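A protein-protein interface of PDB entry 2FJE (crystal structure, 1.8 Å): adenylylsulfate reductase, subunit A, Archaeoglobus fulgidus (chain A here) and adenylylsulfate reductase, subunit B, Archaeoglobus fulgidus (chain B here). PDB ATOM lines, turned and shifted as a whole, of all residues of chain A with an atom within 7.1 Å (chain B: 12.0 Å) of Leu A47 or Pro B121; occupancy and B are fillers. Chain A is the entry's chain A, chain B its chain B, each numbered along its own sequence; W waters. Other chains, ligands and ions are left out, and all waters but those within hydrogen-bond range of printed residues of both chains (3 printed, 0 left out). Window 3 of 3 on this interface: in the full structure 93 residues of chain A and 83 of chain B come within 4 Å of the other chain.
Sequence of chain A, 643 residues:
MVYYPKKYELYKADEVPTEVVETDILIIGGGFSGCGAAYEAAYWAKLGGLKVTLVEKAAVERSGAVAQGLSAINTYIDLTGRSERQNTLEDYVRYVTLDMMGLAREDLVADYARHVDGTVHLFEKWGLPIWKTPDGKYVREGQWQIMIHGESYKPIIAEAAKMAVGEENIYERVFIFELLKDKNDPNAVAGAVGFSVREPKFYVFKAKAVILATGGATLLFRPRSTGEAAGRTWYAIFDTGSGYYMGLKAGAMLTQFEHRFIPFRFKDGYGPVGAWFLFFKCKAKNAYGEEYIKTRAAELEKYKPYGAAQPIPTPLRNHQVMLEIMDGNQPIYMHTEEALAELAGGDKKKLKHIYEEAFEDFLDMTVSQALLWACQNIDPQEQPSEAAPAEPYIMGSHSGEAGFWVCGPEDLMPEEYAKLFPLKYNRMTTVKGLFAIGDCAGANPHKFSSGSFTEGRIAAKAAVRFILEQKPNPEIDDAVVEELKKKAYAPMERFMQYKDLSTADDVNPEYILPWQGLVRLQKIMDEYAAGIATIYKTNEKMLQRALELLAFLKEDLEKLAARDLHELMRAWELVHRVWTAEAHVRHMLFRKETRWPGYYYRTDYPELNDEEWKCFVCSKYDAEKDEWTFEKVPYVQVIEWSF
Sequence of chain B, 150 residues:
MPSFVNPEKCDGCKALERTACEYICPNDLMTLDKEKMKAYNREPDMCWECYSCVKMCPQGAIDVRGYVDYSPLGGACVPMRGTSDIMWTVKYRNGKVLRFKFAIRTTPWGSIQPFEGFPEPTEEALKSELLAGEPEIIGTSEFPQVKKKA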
ATOM      1  N   ALA A  42     -10.214  23.081  -5.046  1.00  0.00           N
ATOM      2  CA  ALA A  42     -11.477  23.701  -5.436  1.00  0.00           C
ATOM      3  C   ALA A  42     -11.945  24.700  -4.380  1.00  0.00           C
ATOM      4  O   ALA A  42     -12.564  25.714  -4.700  1.00  0.00           O
ATOM      5  CB  ALA A  42     -12.538  22.630  -5.650  1.00  0.00           C
ATOM      6  N   TYR A  43     -11.640  24.410  -3.121  1.00  0.00           N
ATOM      7  CA  TYR A  43     -12.043  25.289  -2.028  1.00  0.00           C
ATOM      8  C   TYR A  43     -11.322  26.642  -2.059  1.00  0.00           C
ATOM      9  O   TYR A  43     -11.960  27.696  -2.044  1.00  0.00           O
ATOM     10  CB  TYR A  43     -11.777  24.602  -0.686  1.00  0.00           C
ATOM     11  CG  TYR A  43     -12.134  25.449   0.517  1.00  0.00           C
ATOM     12  CD1 TYR A  43     -13.463  25.641   0.894  1.00  0.00           C
ATOM     13  CD2 TYR A  43     -11.138  26.063   1.277  1.00  0.00           C
ATOM     14  CE1 TYR A  43     -13.789  26.423   2.006  1.00  0.00           C
ATOM     15  CE2 TYR A  43     -11.452  26.844   2.382  1.00  0.00           C
ATOM     16  CZ  TYR A  43     -12.777  27.021   2.743  1.00  0.00           C
ATOM     17  OH  TYR A  43     -13.078  27.792   3.845  1.00  0.00           O
ATOM     18  N   TRP A  44      -9.994  26.612  -2.106  1.00  0.00           N
ATOM     19  CA  TRP A  44      -9.212  27.843  -2.108  1.00  0.00           C
ATOM     20  C   TRP A  44      -9.130  28.563  -3.451  1.00  0.00           C
ATOM     21  O   TRP A  44      -8.944  29.779  -3.490  1.00  0.00           O
ATOM     22  CB  TRP A  44      -7.794  27.564  -1.598  1.00  0.00           C
ATOM     23  CG  TRP A  44      -7.768  26.916  -0.250  1.00  0.00           C
ATOM     24  CD1 TRP A  44      -7.676  25.580   0.018  1.00  0.00           C
ATOM     25  CD2 TRP A  44      -7.894  27.573   1.017  1.00  0.00           C
ATOM     26  NE1 TRP A  44      -7.740  25.363   1.375  1.00  0.00           N
ATOM     27  CE2 TRP A  44      -7.875  26.570   2.011  1.00  0.00           C
ATOM     28  CE3 TRP A  44      -8.025  28.913   1.410  1.00  0.00           C
ATOM     29  CZ2 TRP A  44      -7.981  26.863   3.376  1.00  0.00           C
ATOM     30  CZ3 TRP A  44      -8.131  29.205   2.766  1.00  0.00           C
ATOM     31  CH2 TRP A  44      -8.108  28.182   3.733  1.00  0.00           C
ATOM     32  N   ALA A  45      -9.272  27.821  -4.545  1.00  0.00           N
ATOM     33  CA  ALA A  45      -9.190  28.405  -5.882  1.00  0.00           C
ATOM     34  C   ALA A  45     -10.165  29.561  -6.084  1.00  0.00           C
ATOM     35  O   ALA A  45      -9.900  30.471  -6.867  1.00  0.00           O
ATOM     36  CB  ALA A  45      -9.436  27.330  -6.939  1.00  0.00           C
ATOM     37  N   LYS A  46     -11.289  29.524  -5.377  1.00  0.00           N
ATOM     38  CA  LYS A  46     -12.294  30.572  -5.505  1.00  0.00           C
ATOM     39  C   LYS A  46     -11.728  31.958  -5.184  1.00  0.00           C
ATOM     40  O   LYS A  46     -12.243  32.970  -5.663  1.00  0.00           O
ATOM     41  CB  LYS A  46     -13.490  30.256  -4.597  1.00  0.00           C
ATOM     42  CG  LYS A  46     -14.310  29.048  -5.028  1.00  0.00           C
ATOM     43  CD  LYS A  46     -15.328  28.640  -3.967  1.00  0.00           C
ATOM     44  CE  LYS A  46     -14.639  28.102  -2.722  1.00  0.00           C
ATOM     45  NZ  LYS A  46     -15.586  27.508  -1.749  1.00  0.00           N
ATOM     46  N   LEU A  47     -10.663  32.003  -4.388  1.00  0.00           N
ATOM     47  CA  LEU A  47     -10.043  33.271  -4.017  1.00  0.00           C
ATOM     48  C   LEU A  47      -9.489  34.035  -5.214  1.00  0.00           C
ATOM     49  O   LEU A  47      -9.390  35.262  -5.184  1.00  0.00           O
ATOM     50  CB  LEU A  47      -8.926  33.038  -2.997  1.00  0.00           C
ATOM     51  CG  LEU A  47      -9.379  32.576  -1.612  1.00  0.00           C
ATOM     52  CD1 LEU A  47      -8.168  32.393  -0.716  1.00  0.00           C
ATOM     53  CD2 LEU A  47     -10.334  33.608  -1.017  1.00  0.00           C
ATOM     54  N   GLY A  48      -9.123  33.310  -6.263  1.00  0.00           N
ATOM     55  CA  GLY A  48      -8.591  33.954  -7.447  1.00  0.00           C
ATOM     56  C   GLY A  48      -9.311  33.509  -8.702  1.00  0.00           C
ATOM     57  O   GLY A  48      -8.861  33.790  -9.813  1.00  0.00           O
ATOM     58  N   GLY A  49     -10.435  32.819  -8.530  1.00  0.00           N
ATOM     59  CA  GLY A  49     -11.180  32.335  -9.680  1.00  0.00           C
ATOM     60  C   GLY A  49     -10.302  31.404 -10.500  1.00  0.00           C
ATOM     61  O   GLY A  49     -10.428  31.317 -11.719  1.00  0.00           O
ATOM     62  N   LEU A  50      -9.406  30.701  -9.814  1.00  0.00           N
ATOM     63  CA  LEU A  50      -8.484  29.779 -10.466  1.00  0.00           C
ATOM     64  C   LEU A  50      -9.158  28.520 -10.995  1.00  0.00           C
ATOM     65  O   LEU A  50     -10.125  28.020 -10.417  1.00  0.00           O
ATOM     66  CB  LEU A  50      -7.366  29.378  -9.497  1.00  0.00           C
ATOM     67  CG  LEU A  50      -6.531  30.508  -8.892  1.00  0.00           C
ATOM     68  CD1 LEU A  50      -5.471  29.922  -7.976  1.00  0.00           C
ATOM     69  CD2 LEU A  50      -5.885  31.328  -9.999  1.00  0.00           C
ATOM     70  N   VAL A 464      -2.345  27.036  -4.505  1.00  0.00           N
ATOM     71  CA  VAL A 464      -3.162  28.230  -4.685  1.00  0.00           C
ATOM     72  C   VAL A 464      -2.417  29.418  -4.088  1.00  0.00           C
ATOM     73  O   VAL A 464      -2.380  30.498  -4.679  1.00  0.00           O
ATOM     74  CB  VAL A 464      -4.535  28.094  -3.982  1.00  0.00           C
ATOM     75  CG1 VAL A 464      -5.302  29.415  -4.071  1.00  0.00           C
ATOM     76  CG2 VAL A 464      -5.339  26.984  -4.629  1.00  0.00           C
ATOM     77  N   LEU A 468      -1.233  32.768  -6.181  1.00  0.00           N
ATOM     78  CA  LEU A 468      -1.675  34.103  -5.811  1.00  0.00           C
ATOM     79  C   LEU A 468      -0.558  34.986  -5.268  1.00  0.00           C
ATOM     80  O   LEU A 468      -0.614  36.210  -5.395  1.00  0.00           O
ATOM     81  CB  LEU A 468      -2.822  34.009  -4.801  1.00  0.00           C
ATOM     82  CG  LEU A 468      -4.053  33.257  -5.324  1.00  0.00           C
ATOM     83  CD1 LEU A 468      -5.155  33.289  -4.278  1.00  0.00           C
ATOM     84  CD2 LEU A 468      -4.533  33.889  -6.620  1.00  0.00           C
ATOM     85  N   PRO B 114     -19.328  18.580  -0.749  1.00  0.00           N
ATOM     86  CA  PRO B 114     -17.918  18.786  -0.400  1.00  0.00           C
ATOM     87  C   PRO B 114     -17.564  19.735   0.736  1.00  0.00           C
ATOM     88  O   PRO B 114     -16.801  19.372   1.632  1.00  0.00           O
ATOM     89  CB  PRO B 114     -17.284  19.207  -1.730  1.00  0.00           C
ATOM     90  CG  PRO B 114     -18.426  19.782  -2.502  1.00  0.00           C
ATOM     91  CD  PRO B 114     -19.531  18.811  -2.190  1.00  0.00           C
ATOM     92  N   PHE B 115     -18.114  20.942   0.708  1.00  0.00           N
ATOM     93  CA  PHE B 115     -17.787  21.923   1.735  1.00  0.00           C
ATOM     94  C   PHE B 115     -18.979  22.315   2.601  1.00  0.00           C
ATOM     95  O   PHE B 115     -19.068  23.443   3.080  1.00  0.00           O
ATOM     96  CB  PHE B 115     -17.178  23.150   1.057  1.00  0.00           C
ATOM     97  CG  PHE B 115     -16.172  22.803  -0.010  1.00  0.00           C
ATOM     98  CD1 PHE B 115     -16.383  23.178  -1.334  1.00  0.00           C
ATOM     99  CD2 PHE B 115     -15.028  22.071   0.304  1.00  0.00           C
ATOM    100  CE1 PHE B 115     -15.470  22.827  -2.332  1.00  0.00           C
ATOM    101  CE2 PHE B 115     -14.112  21.716  -0.685  1.00  0.00           C
ATOM    102  CZ  PHE B 115     -14.335  22.096  -2.006  1.00  0.00           C
ATOM    103  N   GLU B 116     -19.881  21.363   2.811  1.00  0.00           N
ATOM    104  CA  GLU B 116     -21.078  21.582   3.616  1.00  0.00           C
ATOM    105  C   GLU B 116     -20.752  22.187   4.979  1.00  0.00           C
ATOM    106  O   GLU B 116     -19.998  21.611   5.763  1.00  0.00           O
ATOM    107  CB  GLU B 116     -21.821  20.257   3.812  1.00  0.00           C
ATOM    108  CG  GLU B 116     -23.132  20.362   4.589  1.00  0.00           C
ATOM    109  CD  GLU B 116     -23.785  19.006   4.821  1.00  0.00           C
ATOM    110  OE1 GLU B 116     -24.902  18.967   5.376  1.00  0.00           O
ATOM    111  OE2 GLU B 116     -23.183  17.975   4.451  1.00  0.00           O
ATOM    112  N   GLY B 117     -21.319  23.358   5.249  1.00  0.00           N
ATOM    113  CA  GLY B 117     -21.101  24.014   6.528  1.00  0.00           C
ATOM    114  C   GLY B 117     -19.799  24.776   6.688  1.00  0.00           C
ATOM    115  O   GLY B 117     -19.616  25.470   7.687  1.00  0.00           O
ATOM    116  N   PHE B 118     -18.892  24.654   5.721  1.00  0.00           N
ATOM    117  CA  PHE B 118     -17.608  25.349   5.799  1.00  0.00           C
ATOM    118  C   PHE B 118     -17.766  26.840   5.549  1.00  0.00           C
ATOM    119  O   PHE B 118     -18.619  27.259   4.772  1.00  0.00           O
ATOM    120  CB  PHE B 118     -16.623  24.829   4.742  1.00  0.00           C
ATOM    121  CG  PHE B 118     -16.170  23.411   4.947  1.00  0.00           C
ATOM    122  CD1 PHE B 118     -16.618  22.653   6.026  1.00  0.00           C
ATOM    123  CD2 PHE B 118     -15.285  22.830   4.041  1.00  0.00           C
ATOM    124  CE1 PHE B 118     -16.190  21.337   6.196  1.00  0.00           C
ATOM    125  CE2 PHE B 118     -14.853  21.518   4.201  1.00  0.00           C
ATOM    126  CZ  PHE B 118     -15.307  20.770   5.281  1.00  0.00           C
ATOM    127  N   PRO B 119     -16.946  27.664   6.214  1.00  0.00           N
ATOM    128  CA  PRO B 119     -17.053  29.105   5.983  1.00  0.00           C
ATOM    129  C   PRO B 119     -16.367  29.372   4.642  1.00  0.00           C
ATOM    130  O   PRO B 119     -15.651  28.508   4.140  1.00  0.00           O
ATOM    131  CB  PRO B 119     -16.289  29.698   7.162  1.00  0.00           C
ATOM    132  CG  PRO B 119     -15.242  28.662   7.441  1.00  0.00           C
ATOM    133  CD  PRO B 119     -16.028  27.371   7.330  1.00  0.00           C
ATOM    134  N   GLU B 120     -16.593  30.539   4.051  1.00  0.00           N
ATOM    135  CA  GLU B 120     -15.954  30.853   2.776  1.00  0.00           C
ATOM    136  C   GLU B 120     -14.465  31.079   3.018  1.00  0.00           C
ATOM    137  O   GLU B 120     -14.063  31.518   4.098  1.00  0.00           O
ATOM    138  CB  GLU B 120     -16.558  32.120   2.160  1.00  0.00           C
ATOM    139  CG  GLU B 120     -18.007  32.000   1.700  1.00  0.00           C
ATOM    140  CD  GLU B 120     -18.193  31.007   0.566  1.00  0.00           C
ATOM    141  OE1 GLU B 120     -17.381  31.018  -0.383  1.00  0.00           O
ATOM    142  OE2 GLU B 120     -19.165  30.223   0.614  1.00  0.00           O
ATOM    143  N   PRO B 121     -13.620  30.764   2.025  1.00  0.00           N
ATOM    144  CA  PRO B 121     -12.186  30.978   2.226  1.00  0.00           C
ATOM    145  C   PRO B 121     -11.886  32.472   2.150  1.00  0.00           C
ATOM    146  O   PRO B 121     -12.660  33.234   1.569  1.00  0.00           O
ATOM    147  CB  PRO B 121     -11.561  30.206   1.068  1.00  0.00           C
ATOM    148  CG  PRO B 121     -12.571  30.395  -0.019  1.00  0.00           C
ATOM    149  CD  PRO B 121     -13.879  30.153   0.709  1.00  0.00           C
ATOM    150  N   THR B 122     -10.774  32.887   2.746  1.00  0.00           N
ATOM    151  CA  THR B 122     -10.373  34.289   2.726  1.00  0.00           C
ATOM    152  C   THR B 122      -8.878  34.364   2.454  1.00  0.00           C
ATOM    153  O   THR B 122      -8.148  33.404   2.703  1.00  0.00           O
ATOM    154  CB  THR B 122     -10.654  34.979   4.072  1.00  0.00           C
ATOM    155  OG1 THR B 122      -9.827  34.397   5.086  1.00  0.00           O
ATOM    156  CG2 THR B 122     -12.115  34.814   4.460  1.00  0.00           C
ATOM    157  N   GLU B 123      -8.418  35.502   1.945  1.00  0.00           N
ATOM    158  CA  GLU B 123      -7.003  35.663   1.652  1.00  0.00           C
ATOM    159  C   GLU B 123      -6.166  35.498   2.912  1.00  0.00           C
ATOM    160  O   GLU B 123      -5.061  34.962   2.866  1.00  0.00           O
ATOM    161  CB  GLU B 123      -6.743  37.032   1.018  1.00  0.00           C
ATOM    162  CG  GLU B 123      -7.318  37.167  -0.383  1.00  0.00           C
ATOM    163  CD  GLU B 123      -6.943  38.475  -1.047  1.00  0.00           C
ATOM    164  OE1 GLU B 123      -5.729  38.752  -1.179  1.00  0.00           O
ATOM    165  OE2 GLU B 123      -7.862  39.227  -1.439  1.00  0.00           O
ATOM    166  N   GLU B 124      -6.696  35.948   4.042  1.00  0.00           N
ATOM    167  CA  GLU B 124      -5.972  35.825   5.296  1.00  0.00           C
ATOM    168  C   GLU B 124      -5.825  34.352   5.667  1.00  0.00           C
ATOM    169  O   GLU B 124      -4.747  33.902   6.058  1.00  0.00           O
ATOM    170  CB  GLU B 124      -6.704  36.566   6.414  1.00  0.00           C
ATOM    171  CG  GLU B 124      -5.937  36.586   7.727  1.00  0.00           C
ATOM    172  CD  GLU B 124      -4.609  37.318   7.618  1.00  0.00           C
ATOM    173  OE1 GLU B 124      -3.832  37.292   8.597  1.00  0.00           O
ATOM    174  OE2 GLU B 124      -4.342  37.924   6.556  1.00  0.00           O
ATOM    175  N   ALA B 125      -6.915  33.606   5.532  1.00  0.00           N
ATOM    176  CA  ALA B 125      -6.918  32.184   5.854  1.00  0.00           C
ATOM    177  C   ALA B 125      -5.951  31.406   4.970  1.00  0.00           C
ATOM    178  O   ALA B 125      -5.340  30.440   5.416  1.00  0.00           O
ATOM    179  CB  ALA B 125      -8.327  31.619   5.704  1.00  0.00           C
ATOM    180  N   LEU B 126      -5.815  31.839   3.721  1.00  0.00           N
ATOM    181  CA  LEU B 126      -4.931  31.182   2.761  1.00  0.00           C
ATOM    182  C   LEU B 126      -3.489  31.116   3.248  1.00  0.00           C
ATOM    183  O   LEU B 126      -2.708  30.275   2.799  1.00  0.00           O
ATOM    184  CB  LEU B 126      -4.979  31.921   1.420  1.00  0.00           C
ATOM    185  CG  LEU B 126      -4.109  31.375   0.283  1.00  0.00           C
ATOM    186  CD1 LEU B 126      -4.554  29.961  -0.073  1.00  0.00           C
ATOM    187  CD2 LEU B 126      -4.224  32.286  -0.930  1.00  0.00           C
ATOM    188  N   LYS B 127      -3.141  31.997   4.179  1.00  0.00           N
ATOM    189  CA  LYS B 127      -1.787  32.041   4.702  1.00  0.00           C
ATOM    190  C   LYS B 127      -1.537  31.184   5.942  1.00  0.00           C
ATOM    191  O   LYS B 127      -0.400  31.072   6.398  1.00  0.00           O
ATOM    192  CB  LYS B 127      -1.412  33.493   4.978  1.00  0.00           C
ATOM    193  CG  LYS B 127      -1.219  34.310   3.712  1.00  0.00           C
ATOM    194  CD  LYS B 127      -0.996  35.785   4.006  1.00  0.00           C
ATOM    195  CE  LYS B 127      -2.271  36.451   4.500  1.00  0.00           C
ATOM    196  NZ  LYS B 127      -2.108  37.925   4.669  1.00  0.00           N
ATOM    197  N   SER B 128      -2.588  30.569   6.477  1.00  0.00           N
ATOM    198  CA  SER B 128      -2.445  29.728   7.663  1.00  0.00           C
ATOM    199  C   SER B 128      -2.216  28.270   7.273  1.00  0.00           C
ATOM    200  O   SER B 128      -2.176  27.930   6.092  1.00  0.00           O
ATOM    201  CB  SER B 128      -3.696  29.814   8.538  1.00  0.00           C
ATOM    202  OG  SER B 128      -4.780  29.123   7.936  1.00  0.00           O
ATOM    203  N   GLU B 129      -2.073  27.412   8.276  1.00  0.00           N
ATOM    204  CA  GLU B 129      -1.852  25.987   8.045  1.00  0.00           C
ATOM    205  C   GLU B 129      -3.181  25.237   7.943  1.00  0.00           C
ATOM    206  O   GLU B 129      -3.204  24.044   7.643  1.00  0.00           O
ATOM    207  CB  GLU B 129      -1.036  25.383   9.193  1.00  0.00           C
ATOM    208  CG  GLU B 129       0.341  25.997   9.417  1.00  0.00           C
ATOM    209  CD  GLU B 129       1.257  25.857   8.214  1.00  0.00           C
ATOM    210  OE1 GLU B 129       1.074  24.909   7.424  1.00  0.00           O
ATOM    211  OE2 GLU B 129       2.175  26.689   8.063  1.00  0.00           O
ATOM    212  N   LEU B 130      -4.283  25.943   8.187  1.00  0.00           N
ATOM    213  CA  LEU B 130      -5.618  25.341   8.157  1.00  0.00           C
ATOM    214  C   LEU B 130      -6.149  24.937   6.786  1.00  0.00           C
ATOM    215  O   LEU B 130      -6.098  25.714   5.833  1.00  0.00           O
ATOM    216  CB  LEU B 130      -6.637  26.290   8.795  1.00  0.00           C
ATOM    217  CG  LEU B 130      -6.444  26.684  10.258  1.00  0.00           C
ATOM    218  CD1 LEU B 130      -7.583  27.595  10.685  1.00  0.00           C
ATOM    219  CD2 LEU B 130      -6.410  25.440  11.128  1.00  0.00           C
ATOM    220  N   LEU B 131      -6.670  23.715   6.703  1.00  0.00           N
ATOM    221  CA  LEU B 131      -7.260  23.217   5.466  1.00  0.00           C
ATOM    222  C   LEU B 131      -8.754  23.496   5.566  1.00  0.00           C
ATOM    223  O   LEU B 131      -9.237  23.937   6.613  1.00  0.00           O
ATOM    224  CB  LEU B 131      -7.028  21.710   5.321  1.00  0.00           C
ATOM    225  CG  LEU B 131      -5.572  21.248   5.229  1.00  0.00           C
ATOM    226  CD1 LEU B 131      -5.529  19.732   5.163  1.00  0.00           C
ATOM    227  CD2 LEU B 131      -4.914  21.846   3.992  1.00  0.00           C
ATOM    228  N   ALA B 132      -9.487  23.237   4.487  1.00  0.00           N
ATOM    229  CA  ALA B 132     -10.925  23.463   4.478  1.00  0.00           C
ATOM    230  C   ALA B 132     -11.599  22.709   5.622  1.00  0.00           C
ATOM    231  O   ALA B 132     -11.376  21.510   5.808  1.00  0.00           O
ATOM    232  CB  ALA B 132     -11.516  23.023   3.141  1.00  0.00           C
ATOM    233  N   GLY B 133     -12.413  23.423   6.394  1.00  0.00           N
ATOM    234  CA  GLY B 133     -13.127  22.810   7.500  1.00  0.00           C
ATOM    235  C   GLY B 133     -12.385  22.752   8.821  1.00  0.00           C
ATOM    236  O   GLY B 133     -12.979  22.417   9.848  1.00  0.00           O
ATOM    237  N   GLU B 134     -11.096  23.075   8.818  1.00  0.00           N
ATOM    238  CA  GLU B 134     -10.321  23.025  10.051  1.00  0.00           C
ATOM    239  C   GLU B 134     -10.414  24.318  10.848  1.00  0.00           C
ATOM    240  O   GLU B 134     -10.660  25.384  10.289  1.00  0.00           O
ATOM    241  CB  GLU B 134      -8.855  22.731   9.747  1.00  0.00           C
ATOM    242  CG  GLU B 134      -8.635  21.441   8.988  1.00  0.00           C
ATOM    243  CD  GLU B 134      -7.170  21.092   8.887  1.00  0.00           C
ATOM    244  OE1 GLU B 134      -6.347  22.028   8.800  1.00  0.00           O
ATOM    245  OE2 GLU B 134      -6.846  19.889   8.889  1.00  0.00           O
ATOM    246  N   GLU B 136     -12.306  22.675  13.032  1.00  0.00           N
ATOM    247  CA  GLU B 136     -13.544  22.004  13.431  1.00  0.00           C
ATOM    248  C   GLU B 136     -13.626  20.518  13.076  1.00  0.00           C
ATOM    249  O   GLU B 136     -13.910  19.679  13.934  1.00  0.00           O
ATOM    250  CB  GLU B 136     -14.762  22.719  12.825  1.00  0.00           C
ATOM    251  CG  GLU B 136     -14.813  24.227  13.068  1.00  0.00           C
ATOM    252  CD  GLU B 136     -13.836  24.990  12.191  1.00  0.00           C
ATOM    253  OE1 GLU B 136     -13.993  24.961  10.953  1.00  0.00           O
ATOM    254  OE2 GLU B 136     -12.910  25.613  12.736  1.00  0.00           O
HETATM  255  O   HOH W   1     -12.803  26.300   6.355  1.00  0.00           O
HETATM  256  O   HOH W   2      -9.302  37.044  -2.918  1.00  0.00           O
HETATM  257  O   HOH W   3     -17.249  27.447   0.063  1.00  0.00           O
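The backbone carbonyl oxygen (O) of Pro B119 lies within hydrogen-bond range of the side-chain hydroxyl (OH) of Tyr A43 (2.7 Å).
The side-chain hydroxyl of Thr B122 sits at hydrogen-bond distance from the backbone NH of Ala B125 (3.1 Å). The side-chain hydroxyl (OG) of Ser B128 is in hydrogen-bond range of the backbone carbonyl oxygen (O) of Ala B125. OG of Ser B128 lies within hydrogen-bond range of N of Leu B130.
Among the printed residues, merely in contact across the chains: Tyr A43 with Phe B115 (3.7 Å), Tyr A43 with Glu B120 (3.7 Å), Tyr A43 with Pro B121 (3.4 Å), Tyr A43 with Ala B132 (3.6 Å), Trp A44 with Pro B121 (3.8 Å), Trp A44 with Ala B125 (3.8 Å), Trp A44 with Leu B126 (3.6 Å), Trp A44 with Leu B130 (3.3 Å), Lys A46 with Pro B121 (3.99 Å), Leu A47 with Pro B121 (3.5 Å), Leu A47 with Thr B122 (3.6 Å), Leu A47 with Leu B126 (3.9 Å) and Leu A468 with Leu B126 (3.6 Å).
Of the printed residues of chain B, Leu A47 touches Pro B121 (3.5 Å), Thr B122 (3.6 Å) and Leu B126 (3.9 Å). Printed residues of chain A within 4 Å of Pro B121: Tyr A43, Trp A44, Lys A46 and Leu A47. No residue of chain B comes within 4 Å of Ala A45. No residue of chain B comes within 4 Å of Gly A48. No residue of chain B comes within 4 Å of Gly A49. No residue of chain B comes within 4 Å of Leu A50. Of the printed residues of chain A, Ala B132 touches Tyr A43 (3.6 Å). Printed residues of chain A within 4 Å of Pro B119: Tyr A43. Glu B136 touches none of the printed residues of chain A. The nearest printed residue of chain B that does not touch Leu A47 is Glu B123 (4.004 Å). The nearest printed residue of chain A that does not touch Pro B121 is Ala A45 (6.2 Å). The nearest printed residue of chain A that does not touch Ala B125 is Leu A47 (6.2 Å).
Printed residues of chain B that touch a printed residue of chain A: Phe B115, Pro B119, Glu B120, Pro B121, Thr B122, Ala B125, Leu B126, Leu B130 and Ala B132. Hydrophobic or aromatic side chains of chain B within 4 Å of the printed part of chain A: Phe B115, Pro B121, Ala B125, Leu B126 and Ala B132.
Water W3 bridges NZ of Lys A46 and OE2 of Glu B120. Water W2 lies within hydrogen-bond range of the backbone carbonyl oxygen (O) of Leu A47 (2.9 Å) and the side-chain carboxylate (OE2) of Glu B123 (3.0 Å). Water W1 lies within hydrogen-bond range of the backbone NH of Gly B133 (2.9 Å) and the side-chain hydroxyl of Tyr A43 (2.9 Å).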
